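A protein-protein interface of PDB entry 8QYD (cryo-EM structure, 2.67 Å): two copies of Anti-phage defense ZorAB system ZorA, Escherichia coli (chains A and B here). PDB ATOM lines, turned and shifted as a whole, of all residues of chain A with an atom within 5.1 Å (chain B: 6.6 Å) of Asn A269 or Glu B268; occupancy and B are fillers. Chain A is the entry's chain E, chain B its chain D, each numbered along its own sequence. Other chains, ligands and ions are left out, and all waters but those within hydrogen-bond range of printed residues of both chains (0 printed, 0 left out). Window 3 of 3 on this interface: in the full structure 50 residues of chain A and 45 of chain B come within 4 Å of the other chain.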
ATOM      1  N   ALA A 262       6.139 -12.911   8.374  1.00  0.00           N
ATOM      2  CA  ALA A 262       5.075 -12.896   9.370  1.00  0.00           C
ATOM      3  C   ALA A 262       3.720 -12.652   8.719  1.00  0.00           C
ATOM      4  O   ALA A 262       2.733 -13.315   9.060  1.00  0.00           O
ATOM      5  CB  ALA A 262       5.360 -11.837  10.434  1.00  0.00           C
ATOM      6  N   SER A 264       2.882 -13.378   5.596  1.00  0.00           N
ATOM      7  CA  SER A 264       2.527 -14.557   4.814  1.00  0.00           C
ATOM      8  C   SER A 264       2.035 -15.691   5.706  1.00  0.00           C
ATOM      9  O   SER A 264       1.034 -16.350   5.395  1.00  0.00           O
ATOM     10  CB  SER A 264       3.722 -15.012   3.978  1.00  0.00           C
ATOM     11  OG  SER A 264       3.373 -16.097   3.139  1.00  0.00           O
ATOM     12  N   GLN A 265       2.721 -15.931   6.826  1.00  0.00           N
ATOM     13  CA  GLN A 265       2.300 -17.010   7.711  1.00  0.00           C
ATOM     14  C   GLN A 265       0.997 -16.670   8.425  1.00  0.00           C
ATOM     15  O   GLN A 265       0.210 -17.573   8.717  1.00  0.00           O
ATOM     16  CB  GLN A 265       3.402 -17.348   8.716  1.00  0.00           C
ATOM     17  CG  GLN A 265       3.735 -16.248   9.698  1.00  0.00           C
ATOM     18  CD  GLN A 265       4.876 -16.626  10.621  1.00  0.00           C
ATOM     19  OE1 GLN A 265       5.393 -17.741  10.563  1.00  0.00           O
ATOM     20  NE2 GLN A 265       5.282 -15.692  11.471  1.00  0.00           N
ATOM     21  N   LYS A 266       0.735 -15.388   8.690  1.00  0.00           N
ATOM     22  CA  LYS A 266      -0.563 -15.011   9.242  1.00  0.00           C
ATOM     23  C   LYS A 266      -1.682 -15.259   8.237  1.00  0.00           C
ATOM     24  O   LYS A 266      -2.759 -15.742   8.605  1.00  0.00           O
ATOM     25  CB  LYS A 266      -0.550 -13.547   9.679  1.00  0.00           C
ATOM     26  CG  LYS A 266      -1.783 -13.130  10.462  1.00  0.00           C
ATOM     27  CD  LYS A 266      -1.916 -11.619  10.530  1.00  0.00           C
ATOM     28  CE  LYS A 266      -2.171 -11.025   9.155  1.00  0.00           C
ATOM     29  NZ  LYS A 266      -3.390 -11.599   8.523  1.00  0.00           N
ATOM     30  N   ILE A 267      -1.446 -14.937   6.962  1.00  0.00           N
ATOM     31  CA  ILE A 267      -2.449 -15.212   5.936  1.00  0.00           C
ATOM     32  C   ILE A 267      -2.700 -16.711   5.824  1.00  0.00           C
ATOM     33  O   ILE A 267      -3.849 -17.161   5.716  1.00  0.00           O
ATOM     34  CB  ILE A 267      -2.026 -14.605   4.585  1.00  0.00           C
ATOM     35  CG1 ILE A 267      -1.850 -13.092   4.710  1.00  0.00           C
ATOM     36  CG2 ILE A 267      -3.041 -14.940   3.504  1.00  0.00           C
ATOM     37  CD1 ILE A 267      -3.112 -12.366   5.116  1.00  0.00           C
ATOM     38  N   GLU A 268      -1.632 -17.510   5.848  1.00  0.00           N
ATOM     39  CA  GLU A 268      -1.813 -18.955   5.773  1.00  0.00           C
ATOM     40  C   GLU A 268      -2.498 -19.508   7.018  1.00  0.00           C
ATOM     41  O   GLU A 268      -3.257 -20.477   6.926  1.00  0.00           O
ATOM     42  CB  GLU A 268      -0.473 -19.648   5.548  1.00  0.00           C
ATOM     43  CG  GLU A 268       0.120 -19.381   4.182  1.00  0.00           C
ATOM     44  CD  GLU A 268       0.915 -20.557   3.670  1.00  0.00           C
ATOM     45  OE1 GLU A 268       0.317 -21.642   3.530  1.00  0.00           O
ATOM     46  OE2 GLU A 268       2.126 -20.399   3.411  1.00  0.00           O
ATOM     47  N   ASN A 269      -2.243 -18.912   8.184  1.00  0.00           N
ATOM     48  CA  ASN A 269      -2.937 -19.326   9.396  1.00  0.00           C
ATOM     49  C   ASN A 269      -4.426 -19.008   9.300  1.00  0.00           C
ATOM     50  O   ASN A 269      -5.268 -19.807   9.728  1.00  0.00           O
ATOM     51  CB  ASN A 269      -2.298 -18.641  10.606  1.00  0.00           C
ATOM     52  CG  ASN A 269      -2.800 -19.185  11.927  1.00  0.00           C
ATOM     53  OD1 ASN A 269      -3.651 -20.068  11.969  1.00  0.00           O
ATOM     54  ND2 ASN A 269      -2.267 -18.656  13.023  1.00  0.00           N
ATOM     55  N   GLU A 270      -4.764 -17.849   8.729  1.00  0.00           N
ATOM     56  CA  GLU A 270      -6.166 -17.529   8.469  1.00  0.00           C
ATOM     57  C   GLU A 270      -6.796 -18.536   7.515  1.00  0.00           C
ATOM     58  O   GLU A 270      -7.941 -18.959   7.713  1.00  0.00           O
ATOM     59  CB  GLU A 270      -6.289 -16.112   7.899  1.00  0.00           C
ATOM     60  CG  GLU A 270      -5.829 -14.975   8.815  1.00  0.00           C
ATOM     61  CD  GLU A 270      -6.608 -14.862  10.122  1.00  0.00           C
ATOM     62  OE1 GLU A 270      -7.526 -15.671  10.375  1.00  0.00           O
ATOM     63  OE2 GLU A 270      -6.293 -13.944  10.910  1.00  0.00           O
ATOM     64  N   ARG A 271      -6.065 -18.924   6.467  1.00  0.00           N
ATOM     65  CA  ARG A 271      -6.588 -19.915   5.531  1.00  0.00           C
ATOM     66  C   ARG A 271      -6.813 -21.258   6.217  1.00  0.00           C
ATOM     67  O   ARG A 271      -7.820 -21.932   5.970  1.00  0.00           O
ATOM     68  CB  ARG A 271      -5.638 -20.074   4.344  1.00  0.00           C
ATOM     69  CG  ARG A 271      -6.331 -20.489   3.055  1.00  0.00           C
ATOM     70  CD  ARG A 271      -5.353 -21.116   2.072  1.00  0.00           C
ATOM     71  NE  ARG A 271      -4.922 -22.440   2.503  1.00  0.00           N
ATOM     72  CZ  ARG A 271      -4.048 -23.194   1.850  1.00  0.00           C
ATOM     73  NH1 ARG A 271      -3.477 -22.778   0.732  1.00  0.00           N
ATOM     74  NH2 ARG A 271      -3.739 -24.394   2.333  1.00  0.00           N
ATOM     75  N   LEU A 272      -5.879 -21.665   7.079  1.00  0.00           N
ATOM     76  CA  LEU A 272      -6.040 -22.913   7.820  1.00  0.00           C
ATOM     77  C   LEU A 272      -7.242 -22.850   8.754  1.00  0.00           C
ATOM     78  O   LEU A 272      -7.989 -23.826   8.884  1.00  0.00           O
ATOM     79  CB  LEU A 272      -4.769 -23.227   8.605  1.00  0.00           C
ATOM     80  CG  LEU A 272      -4.702 -24.615   9.244  1.00  0.00           C
ATOM     81  CD1 LEU A 272      -4.274 -25.656   8.220  1.00  0.00           C
ATOM     82  CD2 LEU A 272      -3.761 -24.613  10.439  1.00  0.00           C
ATOM     83  N   ALA A 273      -7.440 -21.709   9.420  1.00  0.00           N
ATOM     84  CA  ALA A 273      -8.605 -21.549  10.284  1.00  0.00           C
ATOM     85  C   ALA A 273      -9.898 -21.624   9.482  1.00  0.00           C
ATOM     86  O   ALA A 273     -10.876 -22.240   9.923  1.00  0.00           O
ATOM     87  CB  ALA A 273      -8.521 -20.225  11.042  1.00  0.00           C
ATOM     88  N   ASN A 274      -9.921 -21.000   8.302  1.00  0.00           N
ATOM     89  CA  ASN A 274     -11.103 -21.067   7.450  1.00  0.00           C
ATOM     90  C   ASN A 274     -11.384 -22.498   7.008  1.00  0.00           C
ATOM     91  O   ASN A 274     -12.540 -22.937   6.998  1.00  0.00           O
ATOM     92  CB  ASN A 274     -10.928 -20.153   6.238  1.00  0.00           C
ATOM     93  N   GLU B 263       7.264 -14.021  19.068  1.00  0.00           N
ATOM     94  CA  GLU B 263       6.097 -13.424  19.709  1.00  0.00           C
ATOM     95  C   GLU B 263       4.932 -13.306  18.733  1.00  0.00           C
ATOM     96  O   GLU B 263       3.782 -13.602  19.084  1.00  0.00           O
ATOM     97  CB  GLU B 263       6.458 -12.054  20.282  1.00  0.00           C
ATOM     98  CG  GLU B 263       5.269 -11.135  20.487  1.00  0.00           C
ATOM     99  CD  GLU B 263       5.677  -9.686  20.651  1.00  0.00           C
ATOM    100  OE1 GLU B 263       6.893  -9.404  20.635  1.00  0.00           O
ATOM    101  OE2 GLU B 263       4.781  -8.827  20.793  1.00  0.00           O
ATOM    102  N   SER B 264       5.211 -12.875  17.501  1.00  0.00           N
ATOM    103  CA  SER B 264       4.156 -12.763  16.499  1.00  0.00           C
ATOM    104  C   SER B 264       3.551 -14.124  16.182  1.00  0.00           C
ATOM    105  O   SER B 264       2.330 -14.249  16.028  1.00  0.00           O
ATOM    106  CB  SER B 264       4.706 -12.111  15.231  1.00  0.00           C
ATOM    107  OG  SER B 264       3.711 -12.047  14.225  1.00  0.00           O
ATOM    108  N   GLN B 265       4.390 -15.156  16.075  1.00  0.00           N
ATOM    109  CA  GLN B 265       3.886 -16.504  15.832  1.00  0.00           C
ATOM    110  C   GLN B 265       3.011 -16.980  16.984  1.00  0.00           C
ATOM    111  O   GLN B 265       1.970 -17.612  16.765  1.00  0.00           O
ATOM    112  CB  GLN B 265       5.054 -17.465  15.614  1.00  0.00           C
ATOM    113  CG  GLN B 265       5.724 -17.333  14.259  1.00  0.00           C
ATOM    114  CD  GLN B 265       6.584 -18.532  13.917  1.00  0.00           C
ATOM    115  OE1 GLN B 265       6.823 -19.399  14.759  1.00  0.00           O
ATOM    116  NE2 GLN B 265       7.051 -18.593  12.675  1.00  0.00           N
ATOM    117  N   LYS B 266       3.423 -16.690  18.220  1.00  0.00           N
ATOM    118  CA  LYS B 266       2.618 -17.069  19.376  1.00  0.00           C
ATOM    119  C   LYS B 266       1.265 -16.366  19.359  1.00  0.00           C
ATOM    120  O   LYS B 266       0.233 -16.982  19.648  1.00  0.00           O
ATOM    121  CB  LYS B 266       3.377 -16.754  20.665  1.00  0.00           C
ATOM    122  CG  LYS B 266       2.564 -16.937  21.934  1.00  0.00           C
ATOM    123  CD  LYS B 266       3.344 -16.460  23.146  1.00  0.00           C
ATOM    124  CE  LYS B 266       2.564 -16.677  24.430  1.00  0.00           C
ATOM    125  NZ  LYS B 266       3.348 -16.268  25.627  1.00  0.00           N
ATOM    126  N   ILE B 267       1.252 -15.076  19.017  1.00  0.00           N
ATOM    127  CA  ILE B 267      -0.012 -14.344  18.935  1.00  0.00           C
ATOM    128  C   ILE B 267      -0.902 -14.924  17.841  1.00  0.00           C
ATOM    129  O   ILE B 267      -2.116 -15.078  18.025  1.00  0.00           O
ATOM    130  CB  ILE B 267       0.247 -12.842  18.721  1.00  0.00           C
ATOM    131  CG1 ILE B 267       1.065 -12.273  19.881  1.00  0.00           C
ATOM    132  CG2 ILE B 267      -1.064 -12.087  18.567  1.00  0.00           C
ATOM    133  CD1 ILE B 267       0.377 -12.390  21.224  1.00  0.00           C
ATOM    134  N   GLU B 268      -0.318 -15.248  16.685  1.00  0.00           N
ATOM    135  CA  GLU B 268      -1.108 -15.815  15.595  1.00  0.00           C
ATOM    136  C   GLU B 268      -1.696 -17.167  15.980  1.00  0.00           C
ATOM    137  O   GLU B 268      -2.857 -17.460  15.668  1.00  0.00           O
ATOM    138  CB  GLU B 268      -0.254 -15.938  14.334  1.00  0.00           C
ATOM    139  CG  GLU B 268       0.163 -14.602  13.742  1.00  0.00           C
ATOM    140  CD  GLU B 268       1.074 -14.754  12.540  1.00  0.00           C
ATOM    141  OE1 GLU B 268       1.203 -15.886  12.028  1.00  0.00           O
ATOM    142  OE2 GLU B 268       1.664 -13.740  12.110  1.00  0.00           O
ATOM    143  N   ASN B 269      -0.917 -18.005  16.664  1.00  0.00           N
ATOM    144  CA  ASN B 269      -1.437 -19.306  17.073  1.00  0.00           C
ATOM    145  C   ASN B 269      -2.485 -19.168  18.174  1.00  0.00           C
ATOM    146  O   ASN B 269      -3.435 -19.958  18.234  1.00  0.00           O
ATOM    147  CB  ASN B 269      -0.295 -20.215  17.518  1.00  0.00           C
ATOM    148  CG  ASN B 269       0.387 -20.903  16.354  1.00  0.00           C
ATOM    149  OD1 ASN B 269       0.081 -20.632  15.193  1.00  0.00           O
ATOM    150  ND2 ASN B 269       1.315 -21.803  16.659  1.00  0.00           N
ATOM    151  N   GLU B 270      -2.340 -18.172  19.050  1.00  0.00           N
ATOM    152  CA  GLU B 270      -3.384 -17.910  20.036  1.00  0.00           C
ATOM    153  C   GLU B 270      -4.671 -17.457  19.359  1.00  0.00           C
ATOM    154  O   GLU B 270      -5.772 -17.848  19.766  1.00  0.00           O
ATOM    155  CB  GLU B 270      -2.904 -16.869  21.048  1.00  0.00           C
ATOM    156  CG  GLU B 270      -4.017 -16.219  21.853  1.00  0.00           C
ATOM    157  CD  GLU B 270      -3.530 -15.053  22.689  1.00  0.00           C
ATOM    158  OE1 GLU B 270      -2.308 -14.798  22.700  1.00  0.00           O
ATOM    159  OE2 GLU B 270      -4.368 -14.391  23.335  1.00  0.00           O
ATOM    160  N   ARG B 271      -4.551 -16.633  18.317  1.00  0.00           N
ATOM    161  CA  ARG B 271      -5.725 -16.245  17.541  1.00  0.00           C
ATOM    162  C   ARG B 271      -6.352 -17.458  16.863  1.00  0.00           C
ATOM    163  O   ARG B 271      -7.581 -17.560  16.769  1.00  0.00           O
ATOM    164  CB  ARG B 271      -5.342 -15.175  16.515  1.00  0.00           C
ATOM    165  CG  ARG B 271      -6.514 -14.523  15.782  1.00  0.00           C
ATOM    166  CD  ARG B 271      -6.890 -15.288  14.523  1.00  0.00           C
ATOM    167  NE  ARG B 271      -5.722 -15.588  13.705  1.00  0.00           N
ATOM    168  CZ  ARG B 271      -5.703 -16.479  12.723  1.00  0.00           C
ATOM    169  NH1 ARG B 271      -6.773 -17.196  12.420  1.00  0.00           N
ATOM    170  NH2 ARG B 271      -4.584 -16.652  12.027  1.00  0.00           N
ATOM    171  N   LEU B 272      -5.523 -18.380  16.369  1.00  0.00           N
ATOM    172  CA  LEU B 272      -6.046 -19.619  15.799  1.00  0.00           C
ATOM    173  C   LEU B 272      -6.804 -20.434  16.840  1.00  0.00           C
ATOM    174  O   LEU B 272      -7.861 -21.002  16.546  1.00  0.00           O
ATOM    175  CB  LEU B 272      -4.914 -20.449  15.197  1.00  0.00           C
ATOM    176  CG  LEU B 272      -5.335 -21.804  14.623  1.00  0.00           C
ATOM    177  CD1 LEU B 272      -5.988 -21.660  13.260  1.00  0.00           C
ATOM    178  CD2 LEU B 272      -4.138 -22.740  14.546  1.00  0.00           C
ATOM    179  N   ALA B 273      -6.270 -20.512  18.060  1.00  0.00           N
ATOM    180  CA  ALA B 273      -6.968 -21.218  19.130  1.00  0.00           C
ATOM    181  C   ALA B 273      -8.302 -20.553  19.449  1.00  0.00           C
ATOM    182  O   ALA B 273      -9.311 -21.235  19.664  1.00  0.00           O
ATOM    183  CB  ALA B 273      -6.089 -21.285  20.378  1.00  0.00           C
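Gln A265 touches Glu B268 (CG to OE1, 3.5 Å).
O of Lys A266 touches NH2 of Arg B271 (3.98 Å).
Asn B269 touches Asn A269 (OD1 to ND2, 3.8 Å).
Leu B272 touches Asn A269.
Ala A273 touches Arg B271 (CB to NH1, 3.8 Å).
CD1 of Leu B272 touches CB of Ala A273, 3.7 Å away.
The side-chain hydroxyl (OG) of Ser B264 lies within hydrogen-bond range of the side-chain carboxylate (OE2) of Glu B268, 3.4 Å away.
Printed residues of chain B within 4 Å of Lys A266: Glu B268 (3.3 Å) and Arg B271 (3.98 Å).
Asn A269 touches four residues of chain B.
Of the printed residues of chain B, Glu A270 touches Arg B271 (2.7 Å).
Of the printed residues of chain B, Ala A273 touches Arg B271 and Leu B272.
Glu B263 touches none of the printed residues of chain A.
Of the printed residues of chain A, Gln B265 touches Gln A265 (2.8 Å).
Glu B268 touches four residues of chain A.
Printed residues of chain A within 4 Å of Arg B271: Lys A266, Asn A269, Glu A270 and Ala A273.
The nearest residue of chain B that does not touch Asn A269 is Gln B265 (5.7 Å).
Asn A269 touches Glu B268, but with the chains exchanged Glu A268 does not touch Asn B269 (8.6 Å).
Asn A269 touches Leu B272, but with the chains exchanged Leu A272 does not touch Asn B269 (7.3 Å).
Glu A270 touches Arg B271, but with the chains exchanged Arg A271 does not touch Glu B270 (13.0 Å).
Ala A273 touches Leu B272, but with the chains exchanged Leu A272 does not touch Ala B273 (9.0 Å).
Positions printed for both chains: 264, 265, 266, 267, 268, 269, 270, 271, 272 and 273.
NE2 of Gln B265 sits at hydrogen-bond distance from OE1 of Gln A265, 2.8 Å away.
OE1 of Glu B268 sits at hydrogen-bond distance from N of Lys A266.
The backbone carbonyl oxygen of Glu B268 sits at hydrogen-bond distance from the side-chain amide nitrogen of Asn A269, 3.0 Å away.
ND2 of Asn A269 lies close to NH2 of Arg B271 (3.2 Å).
The guanidinium group (NH1) of Arg B271 lies within salt-bridge range of the side-chain carboxylate (OE1) of Glu A270 (2.7 Å).
The backbone carbonyl oxygen (O) of Ala A262 lies close to the side-chain carboxylate (OE2) of Glu B268, 3.3 Å away.
Of the 11 printed residues of chain B, 5 touch a printed residue of chain A.
Hydrophobic or aromatic side chains of chain A within 4 Å of the printed part of chain B: Ala A273.
Among the printed residues, Asp or Glu carboxylates within 4 Å of a Lys or Arg side-chain nitrogen of the other chain: Glu A270 with Arg B271 (2.7 Å).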
